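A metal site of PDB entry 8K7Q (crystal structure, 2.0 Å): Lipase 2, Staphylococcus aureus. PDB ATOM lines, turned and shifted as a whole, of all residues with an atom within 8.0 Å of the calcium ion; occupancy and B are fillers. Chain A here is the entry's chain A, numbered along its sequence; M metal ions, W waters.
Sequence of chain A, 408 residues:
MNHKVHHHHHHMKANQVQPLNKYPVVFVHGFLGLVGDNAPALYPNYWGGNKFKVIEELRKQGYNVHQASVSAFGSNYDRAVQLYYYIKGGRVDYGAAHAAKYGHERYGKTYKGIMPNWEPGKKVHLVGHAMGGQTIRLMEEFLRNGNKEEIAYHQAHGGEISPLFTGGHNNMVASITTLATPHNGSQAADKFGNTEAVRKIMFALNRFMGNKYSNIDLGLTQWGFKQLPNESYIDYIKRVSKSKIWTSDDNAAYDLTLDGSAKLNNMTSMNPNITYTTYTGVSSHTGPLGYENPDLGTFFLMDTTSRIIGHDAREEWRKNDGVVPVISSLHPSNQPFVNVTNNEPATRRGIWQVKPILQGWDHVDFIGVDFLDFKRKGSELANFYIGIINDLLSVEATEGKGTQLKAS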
ATOM      1  N   LYS A  51     -11.416 -18.056  13.153  1.00  0.00           N
ATOM      2  CA  LYS A  51     -10.903 -19.387  13.439  1.00  0.00           C
ATOM      3  C   LYS A  51      -9.441 -19.320  13.884  1.00  0.00           C
ATOM      4  O   LYS A  51      -9.072 -19.998  14.821  1.00  0.00           O
ATOM      5  CB  LYS A  51     -11.122 -20.324  12.249  1.00  0.00           C
ATOM      6  CG  LYS A  51     -12.590 -20.568  11.971  1.00  0.00           C
ATOM      7  CD  LYS A  51     -12.856 -21.602  10.921  1.00  0.00           C
ATOM      8  CE  LYS A  51     -14.347 -21.825  10.760  1.00  0.00           C
ATOM      9  NZ  LYS A  51     -14.633 -22.940   9.803  1.00  0.00           N
ATOM     10  N   SER A 283     -13.583 -29.433  -2.838  1.00  0.00           N
ATOM     11  CA  SER A 283     -14.784 -29.324  -2.028  1.00  0.00           C
ATOM     12  C   SER A 283     -15.977 -29.672  -2.896  1.00  0.00           C
ATOM     13  O   SER A 283     -17.098 -29.184  -2.686  1.00  0.00           O
ATOM     14  CB  SER A 283     -14.900 -27.916  -1.463  1.00  0.00           C
ATOM     15  OG  SER A 283     -16.007 -27.827  -0.577  1.00  0.00           O
ATOM     16  N   ASP A 295     -19.663 -30.036  -2.251  1.00  0.00           N
ATOM     17  CA  ASP A 295     -19.950 -30.716  -0.993  1.00  0.00           C
ATOM     18  C   ASP A 295     -20.831 -29.831  -0.114  1.00  0.00           C
ATOM     19  O   ASP A 295     -20.766 -28.591  -0.207  1.00  0.00           O
ATOM     20  CB  ASP A 295     -18.662 -31.004  -0.209  1.00  0.00           C
ATOM     21  CG  ASP A 295     -17.705 -31.930  -0.922  1.00  0.00           C
ATOM     22  OD1 ASP A 295     -18.119 -32.570  -1.934  1.00  0.00           O
ATOM     23  OD2 ASP A 295     -16.524 -31.999  -0.466  1.00  0.00           O
ATOM     24  N   LEU A 296     -21.659 -30.458   0.725  1.00  0.00           N
ATOM     25  CA  LEU A 296     -22.225 -29.769   1.878  1.00  0.00           C
ATOM     26  C   LEU A 296     -21.025 -29.182   2.593  1.00  0.00           C
ATOM     27  O   LEU A 296     -20.028 -29.868   2.805  1.00  0.00           O
ATOM     28  CB  LEU A 296     -22.903 -30.811   2.778  1.00  0.00           C
ATOM     29  CG  LEU A 296     -24.363 -31.206   2.541  1.00  0.00           C
ATOM     30  CD1 LEU A 296     -24.793 -31.052   1.076  1.00  0.00           C
ATOM     31  CD2 LEU A 296     -24.591 -32.645   2.984  1.00  0.00           C
ATOM     32  N   GLY A 297     -21.076 -27.904   2.954  1.00  0.00           N
ATOM     33  CA  GLY A 297     -19.869 -27.467   3.630  1.00  0.00           C
ATOM     34  C   GLY A 297     -19.040 -26.500   2.785  1.00  0.00           C
ATOM     35  O   GLY A 297     -18.248 -25.731   3.328  1.00  0.00           O
ATOM     36  N   THR A 298     -19.209 -26.591   1.443  1.00  0.00           N
ATOM     37  CA  THR A 298     -18.761 -25.521   0.571  1.00  0.00           C
ATOM     38  C   THR A 298     -19.517 -24.288   1.019  1.00  0.00           C
ATOM     39  O   THR A 298     -20.740 -24.332   1.147  1.00  0.00           O
ATOM     40  CB  THR A 298     -19.162 -25.795  -0.879  1.00  0.00           C
ATOM     41  OG1 THR A 298     -18.631 -27.077  -1.224  1.00  0.00           O
ATOM     42  CG2 THR A 298     -18.657 -24.748  -1.843  1.00  0.00           C
ATOM     43  N   PHE A 299     -18.793 -23.214   1.339  1.00  0.00           N
ATOM     44  CA  PHE A 299     -19.457 -21.972   1.696  1.00  0.00           C
ATOM     45  C   PHE A 299     -20.511 -21.648   0.641  1.00  0.00           C
ATOM     46  O   PHE A 299     -20.210 -21.643  -0.562  1.00  0.00           O
ATOM     47  CB  PHE A 299     -18.417 -20.862   1.821  1.00  0.00           C
ATOM     48  CG  PHE A 299     -18.989 -19.593   2.399  1.00  0.00           C
ATOM     49  CD1 PHE A 299     -19.375 -19.537   3.741  1.00  0.00           C
ATOM     50  CD2 PHE A 299     -19.154 -18.475   1.609  1.00  0.00           C
ATOM     51  CE1 PHE A 299     -19.912 -18.371   4.267  1.00  0.00           C
ATOM     52  CE2 PHE A 299     -19.698 -17.313   2.140  1.00  0.00           C
ATOM     53  CZ  PHE A 299     -20.080 -17.260   3.465  1.00  0.00           C
ATOM     54  N   PHE A 300     -21.744 -21.381   1.100  1.00  0.00           N
ATOM     55  CA  PHE A 300     -22.938 -21.415   0.260  1.00  0.00           C
ATOM     56  C   PHE A 300     -22.850 -20.423  -0.907  1.00  0.00           C
ATOM     57  O   PHE A 300     -23.443 -20.680  -1.949  1.00  0.00           O
ATOM     58  CB  PHE A 300     -24.238 -21.156   1.054  1.00  0.00           C
ATOM     59  CG  PHE A 300     -24.411 -19.728   1.539  1.00  0.00           C
ATOM     60  CD1 PHE A 300     -23.693 -19.255   2.627  1.00  0.00           C
ATOM     61  CD2 PHE A 300     -25.293 -18.865   0.893  1.00  0.00           C
ATOM     62  CE1 PHE A 300     -23.849 -17.945   3.058  1.00  0.00           C
ATOM     63  CE2 PHE A 300     -25.445 -17.548   1.336  1.00  0.00           C
ATOM     64  CZ  PHE A 300     -24.724 -17.084   2.420  1.00  0.00           C
ATOM     65  N   MET A 302     -20.667 -20.063  -2.922  1.00  0.00           N
ATOM     66  CA  MET A 302     -19.936 -20.657  -4.036  1.00  0.00           C
ATOM     67  C   MET A 302     -20.695 -21.839  -4.644  1.00  0.00           C
ATOM     68  O   MET A 302     -20.145 -22.543  -5.493  1.00  0.00           O
ATOM     69  CB  MET A 302     -18.555 -21.127  -3.572  1.00  0.00           C
ATOM     70  CG  MET A 302     -17.619 -19.971  -3.308  1.00  0.00           C
ATOM     71  SD  MET A 302     -15.940 -20.455  -2.862  1.00  0.00           S
ATOM     72  CE  MET A 302     -16.196 -21.314  -1.309  1.00  0.00           C
ATOM     73  N   ASP A 321     -12.660 -26.111  -5.734  1.00  0.00           N
ATOM     74  CA  ASP A 321     -12.743 -25.708  -4.335  1.00  0.00           C
ATOM     75  C   ASP A 321     -13.949 -24.785  -4.117  1.00  0.00           C
ATOM     76  O   ASP A 321     -14.009 -24.066  -3.109  1.00  0.00           O
ATOM     77  CB  ASP A 321     -11.464 -25.003  -3.889  1.00  0.00           C
ATOM     78  CG  ASP A 321     -11.292 -23.603  -4.479  1.00  0.00           C
ATOM     79  OD1 ASP A 321     -12.183 -23.145  -5.258  1.00  0.00           O
ATOM     80  OD2 ASP A 321     -10.246 -22.988  -4.199  1.00  0.00           O
ATOM     81  N   GLY A 360     -11.919 -31.562   1.305  1.00  0.00           N
ATOM     82  CA  GLY A 360     -12.972 -30.872   2.035  1.00  0.00           C
ATOM     83  C   GLY A 360     -12.735 -29.362   2.226  1.00  0.00           C
ATOM     84  O   GLY A 360     -13.587 -28.666   2.786  1.00  0.00           O
ATOM     85  N   TRP A 361     -11.562 -28.867   1.811  1.00  0.00           N
ATOM     86  CA  TRP A 361     -11.245 -27.444   1.968  1.00  0.00           C
ATOM     87  C   TRP A 361     -11.723 -26.679   0.743  1.00  0.00           C
ATOM     88  O   TRP A 361     -11.189 -26.865  -0.368  1.00  0.00           O
ATOM     89  CB  TRP A 361      -9.736 -27.221   2.114  1.00  0.00           C
ATOM     90  CG  TRP A 361      -9.139 -27.596   3.442  1.00  0.00           C
ATOM     91  CD1 TRP A 361      -9.305 -28.767   4.129  1.00  0.00           C
ATOM     92  CD2 TRP A 361      -8.196 -26.801   4.195  1.00  0.00           C
ATOM     93  NE1 TRP A 361      -8.553 -28.740   5.279  1.00  0.00           N
ATOM     94  CE2 TRP A 361      -7.859 -27.560   5.343  1.00  0.00           C
ATOM     95  CE3 TRP A 361      -7.610 -25.538   4.008  1.00  0.00           C
ATOM     96  CZ2 TRP A 361      -6.949 -27.097   6.291  1.00  0.00           C
ATOM     97  CZ3 TRP A 361      -6.697 -25.085   4.952  1.00  0.00           C
ATOM     98  CH2 TRP A 361      -6.385 -25.851   6.079  1.00  0.00           C
ATOM     99  N   ASP A 362     -12.734 -25.808   0.943  1.00  0.00           N
ATOM    100  CA  ASP A 362     -13.169 -24.938  -0.137  1.00  0.00           C
ATOM    101  C   ASP A 362     -12.255 -23.721  -0.174  1.00  0.00           C
ATOM    102  O   ASP A 362     -11.367 -23.549   0.678  1.00  0.00           O
ATOM    103  CB  ASP A 362     -14.667 -24.593  -0.034  1.00  0.00           C
ATOM    104  CG  ASP A 362     -15.016 -23.688   1.141  1.00  0.00           C
ATOM    105  OD1 ASP A 362     -14.211 -22.778   1.477  1.00  0.00           O
ATOM    106  OD2 ASP A 362     -16.113 -23.864   1.693  1.00  0.00           O
ATOM    107  N   HIS A 363     -12.491 -22.862  -1.159  1.00  0.00           N
ATOM    108  CA  HIS A 363     -11.690 -21.690  -1.443  1.00  0.00           C
ATOM    109  C   HIS A 363     -11.480 -20.821  -0.207  1.00  0.00           C
ATOM    110  O   HIS A 363     -10.375 -20.310   0.012  1.00  0.00           O
ATOM    111  CB  HIS A 363     -12.384 -20.916  -2.562  1.00  0.00           C
ATOM    112  CG  HIS A 363     -11.505 -19.899  -3.186  1.00  0.00           C
ATOM    113  ND1 HIS A 363     -10.456 -20.240  -3.997  1.00  0.00           N
ATOM    114  CD2 HIS A 363     -11.545 -18.561  -3.155  1.00  0.00           C
ATOM    115  CE1 HIS A 363      -9.861 -19.127  -4.424  1.00  0.00           C
ATOM    116  NE2 HIS A 363     -10.507 -18.089  -3.927  1.00  0.00           N
ATOM    117  N   VAL A 364     -12.533 -20.653   0.609  1.00  0.00           N
ATOM    118  CA  VAL A 364     -12.411 -19.718   1.721  1.00  0.00           C
ATOM    119  C   VAL A 364     -12.065 -20.433   3.031  1.00  0.00           C
ATOM    120  O   VAL A 364     -11.691 -19.768   3.989  1.00  0.00           O
ATOM    121  CB  VAL A 364     -13.628 -18.785   1.858  1.00  0.00           C
ATOM    122  CG1 VAL A 364     -13.844 -17.955   0.595  1.00  0.00           C
ATOM    123  CG2 VAL A 364     -14.903 -19.519   2.242  1.00  0.00           C
ATOM    124  N   ASP A 365     -12.107 -21.773   3.056  1.00  0.00           N
ATOM    125  CA  ASP A 365     -11.610 -22.506   4.219  1.00  0.00           C
ATOM    126  C   ASP A 365     -10.122 -22.192   4.428  1.00  0.00           C
ATOM    127  O   ASP A 365      -9.639 -22.196   5.561  1.00  0.00           O
ATOM    128  CB  ASP A 365     -11.865 -24.012   4.137  1.00  0.00           C
ATOM    129  CG  ASP A 365     -13.339 -24.401   4.206  1.00  0.00           C
ATOM    130  OD1 ASP A 365     -14.071 -23.790   5.031  1.00  0.00           O
ATOM    131  OD2 ASP A 365     -13.763 -25.320   3.462  1.00  0.00           O
ATOM    132  N   PHE A 366      -9.396 -21.888   3.340  1.00  0.00           N
ATOM    133  CA  PHE A 366      -7.978 -21.556   3.466  1.00  0.00           C
ATOM    134  C   PHE A 366      -7.731 -20.302   4.314  1.00  0.00           C
ATOM    135  O   PHE A 366      -6.617 -20.137   4.811  1.00  0.00           O
ATOM    136  CB  PHE A 366      -7.319 -21.315   2.101  1.00  0.00           C
ATOM    137  CG  PHE A 366      -7.034 -22.597   1.380  1.00  0.00           C
ATOM    138  CD1 PHE A 366      -5.857 -23.288   1.611  1.00  0.00           C
ATOM    139  CD2 PHE A 366      -7.986 -23.162   0.537  1.00  0.00           C
ATOM    140  CE1 PHE A 366      -5.620 -24.505   0.970  1.00  0.00           C
ATOM    141  CE2 PHE A 366      -7.751 -24.371  -0.099  1.00  0.00           C
ATOM    142  CZ  PHE A 366      -6.561 -25.038   0.112  1.00  0.00           C
ATOM    143  N   VAL A 369     -12.756 -18.204   6.879  1.00  0.00           N
ATOM    144  CA  VAL A 369     -13.900 -17.310   6.971  1.00  0.00           C
ATOM    145  C   VAL A 369     -15.183 -18.100   6.789  1.00  0.00           C
ATOM    146  O   VAL A 369     -16.257 -17.526   6.832  1.00  0.00           O
ATOM    147  CB  VAL A 369     -13.832 -16.092   6.017  1.00  0.00           C
ATOM    148  CG1 VAL A 369     -12.602 -15.236   6.271  1.00  0.00           C
ATOM    149  CG2 VAL A 369     -13.863 -16.503   4.567  1.00  0.00           C
ATOM    150  N   ASP A 370     -15.098 -19.419   6.591  1.00  0.00           N
ATOM    151  CA  ASP A 370     -16.341 -20.176   6.436  1.00  0.00           C
ATOM    152  C   ASP A 370     -16.901 -20.458   7.827  1.00  0.00           C
ATOM    153  O   ASP A 370     -16.689 -21.544   8.370  1.00  0.00           O
ATOM    154  CB  ASP A 370     -16.152 -21.433   5.602  1.00  0.00           C
ATOM    155  CG  ASP A 370     -17.439 -22.203   5.375  1.00  0.00           C
ATOM    156  OD1 ASP A 370     -18.482 -21.860   6.007  1.00  0.00           O
ATOM    157  OD2 ASP A 370     -17.437 -23.103   4.537  1.00  0.00           O
ATOM    158  N   PHE A 371     -17.660 -19.487   8.380  1.00  0.00           N
ATOM    159  CA  PHE A 371     -18.185 -19.589   9.741  1.00  0.00           C
ATOM    160  C   PHE A 371     -19.312 -20.618   9.787  1.00  0.00           C
ATOM    161  O   PHE A 371     -19.744 -20.980  10.878  1.00  0.00           O
ATOM    162  CB  PHE A 371     -18.682 -18.245  10.297  1.00  0.00           C
ATOM    163  CG  PHE A 371     -19.848 -17.666   9.539  1.00  0.00           C
ATOM    164  CD1 PHE A 371     -19.650 -16.911   8.387  1.00  0.00           C
ATOM    165  CD2 PHE A 371     -21.153 -17.989   9.892  1.00  0.00           C
ATOM    166  CE1 PHE A 371     -20.720 -16.427   7.647  1.00  0.00           C
ATOM    167  CE2 PHE A 371     -22.226 -17.497   9.155  1.00  0.00           C
ATOM    168  CZ  PHE A 371     -22.008 -16.730   8.042  1.00  0.00           C
ATOM    169  N   LEU A 372     -19.804 -21.084   8.640  1.00  0.00           N
ATOM    170  CA  LEU A 372     -20.869 -22.081   8.628  1.00  0.00           C
ATOM    171  C   LEU A 372     -20.323 -23.501   8.626  1.00  0.00           C
ATOM    172  O   LEU A 372     -21.112 -24.438   8.590  1.00  0.00           O
ATOM    173  CB  LEU A 372     -21.689 -21.907   7.340  1.00  0.00           C
ATOM    174  CG  LEU A 372     -22.918 -20.998   7.347  1.00  0.00           C
ATOM    175  CD1 LEU A 372     -23.324 -20.491   8.724  1.00  0.00           C
ATOM    176  CD2 LEU A 372     -22.837 -19.915   6.300  1.00  0.00           C
ATOM    177  N   ASP A 373     -18.997 -23.704   8.608  1.00  0.00           N
ATOM    178  CA  ASP A 373     -18.439 -25.023   8.365  1.00  0.00           C
ATOM    179  C   ASP A 373     -17.665 -25.512   9.598  1.00  0.00           C
ATOM    180  O   ASP A 373     -16.481 -25.217   9.769  1.00  0.00           O
ATOM    181  CB  ASP A 373     -17.533 -25.036   7.134  1.00  0.00           C
ATOM    182  CG  ASP A 373     -17.001 -26.403   6.702  1.00  0.00           C
ATOM    183  OD1 ASP A 373     -17.193 -27.390   7.466  1.00  0.00           O
ATOM    184  OD2 ASP A 373     -16.421 -26.492   5.601  1.00  0.00           O
ATOM    185  N   PHE A 374     -18.338 -26.327  10.423  1.00  0.00           N
ATOM    186  CA  PHE A 374     -17.811 -26.701  11.731  1.00  0.00           C
ATOM    187  C   PHE A 374     -16.755 -27.809  11.588  1.00  0.00           C
ATOM    188  O   PHE A 374     -15.957 -28.014  12.501  1.00  0.00           O
ATOM    189  CB  PHE A 374     -18.973 -26.954  12.696  1.00  0.00           C
ATOM    190  CG  PHE A 374     -18.569 -27.138  14.138  1.00  0.00           C
ATOM    191  CD1 PHE A 374     -17.941 -26.116  14.849  1.00  0.00           C
ATOM    192  CD2 PHE A 374     -18.786 -28.348  14.781  1.00  0.00           C
ATOM    193  CE1 PHE A 374     -17.558 -26.289  16.178  1.00  0.00           C
ATOM    194  CE2 PHE A 374     -18.400 -28.530  16.105  1.00  0.00           C
ATOM    195  CZ  PHE A 374     -17.794 -27.494  16.798  1.00  0.00           C
ATOM    196  N   LYS A 375     -16.692 -28.461  10.432  1.00  0.00           N
ATOM    197  CA  LYS A 375     -15.659 -29.467  10.171  1.00  0.00           C
ATOM    198  C   LYS A 375     -14.274 -28.835  10.084  1.00  0.00           C
ATOM    199  O   LYS A 375     -13.269 -29.511  10.278  1.00  0.00           O
ATOM    200  CB  LYS A 375     -15.947 -30.209   8.856  1.00  0.00           C
ATOM    201  CG  LYS A 375     -17.256 -30.985   8.780  1.00  0.00           C
ATOM    202  CD  LYS A 375     -17.748 -31.260   7.355  1.00  0.00           C
ATOM    203  CE  LYS A 375     -16.769 -32.021   6.485  1.00  0.00           C
ATOM    204  NZ  LYS A 375     -16.390 -33.341   7.048  1.00  0.00           N
ATOM    205  N   ARG A 376     -14.196 -27.541   9.751  1.00  0.00           N
ATOM    206  CA  ARG A 376     -12.894 -26.919   9.559  1.00  0.00           C
ATOM    207  C   ARG A 376     -12.606 -26.098  10.825  1.00  0.00           C
ATOM    208  O   ARG A 376     -13.182 -25.014  11.006  1.00  0.00           O
ATOM    209  CB  ARG A 376     -12.950 -26.049   8.303  1.00  0.00           C
ATOM    210  CG  ARG A 376     -13.278 -26.789   7.009  1.00  0.00           C
ATOM    211  CD  ARG A 376     -12.050 -27.417   6.343  1.00  0.00           C
ATOM    212  NE  ARG A 376     -11.393 -28.498   7.067  1.00  0.00           N
ATOM    213  CZ  ARG A 376     -11.781 -29.783   7.040  1.00  0.00           C
ATOM    214  NH1 ARG A 376     -11.056 -30.704   7.647  1.00  0.00           N
ATOM    215  NH2 ARG A 376     -12.867 -30.135   6.372  1.00  0.00           N
HETATM  216 CA    CA M   1     -16.109 -24.988   3.820  1.00  0.00          CA
HETATM  217  O   HOH W   1     -15.851 -26.986   2.313  1.00  0.00           O
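The side-chain amino group (NZ) of Lys 51 sits at hydrogen-bond distance from the backbone carbonyl oxygen (O) of Asp 373 (2.9 Å).
OD2 of Asp 362 lies close to N of Phe 299 (2.8 Å).
The backbone NH (N) of Phe 299 lies close to the side-chain carboxylate (OD2) of Asp 370.
OD1 of Asp 370 lies within hydrogen-bond range of N of Leu 372.
The side-chain carboxylate of Asp 373 sits at hydrogen-bond distance from the backbone NH of Lys 375, at 3.2 Å.
The side-chain carboxylate of Asp 362 is in hydrogen-bond range of the backbone NH of Val 364 (2.8 Å).
NZ of Lys 51 is in hydrogen-bond range of O of Asp 370, 2.9 Å away.
Within 4 Å of the calcium ion: Gly 297, Asp 362, Asp 365, Asp 370 and Asp 373.
The calcium ion is bound by O of Gly 297 (2.3 Å).
The side-chain carboxylate (OD2) of Asp 373 binds the calcium ion.
The calcium ion is bound by OD2 of Asp 365 (2.4 Å).
The calcium ion is bound by OD2 of Asp 362 (2.4 Å).
OD2 of Asp 370 is bound to the calcium ion (2.4 Å).
The calcium ion is bound by water W1 (2.5 Å).
The calcium ion is bound by the side-chain carboxylate (OD1) of Asp 365 (2.7 Å).
Water W1 lies within hydrogen-bond range of the backbone carbonyl oxygen of Gly 360, the side-chain hydroxyl of Ser 283 and the backbone NH of Thr 298.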
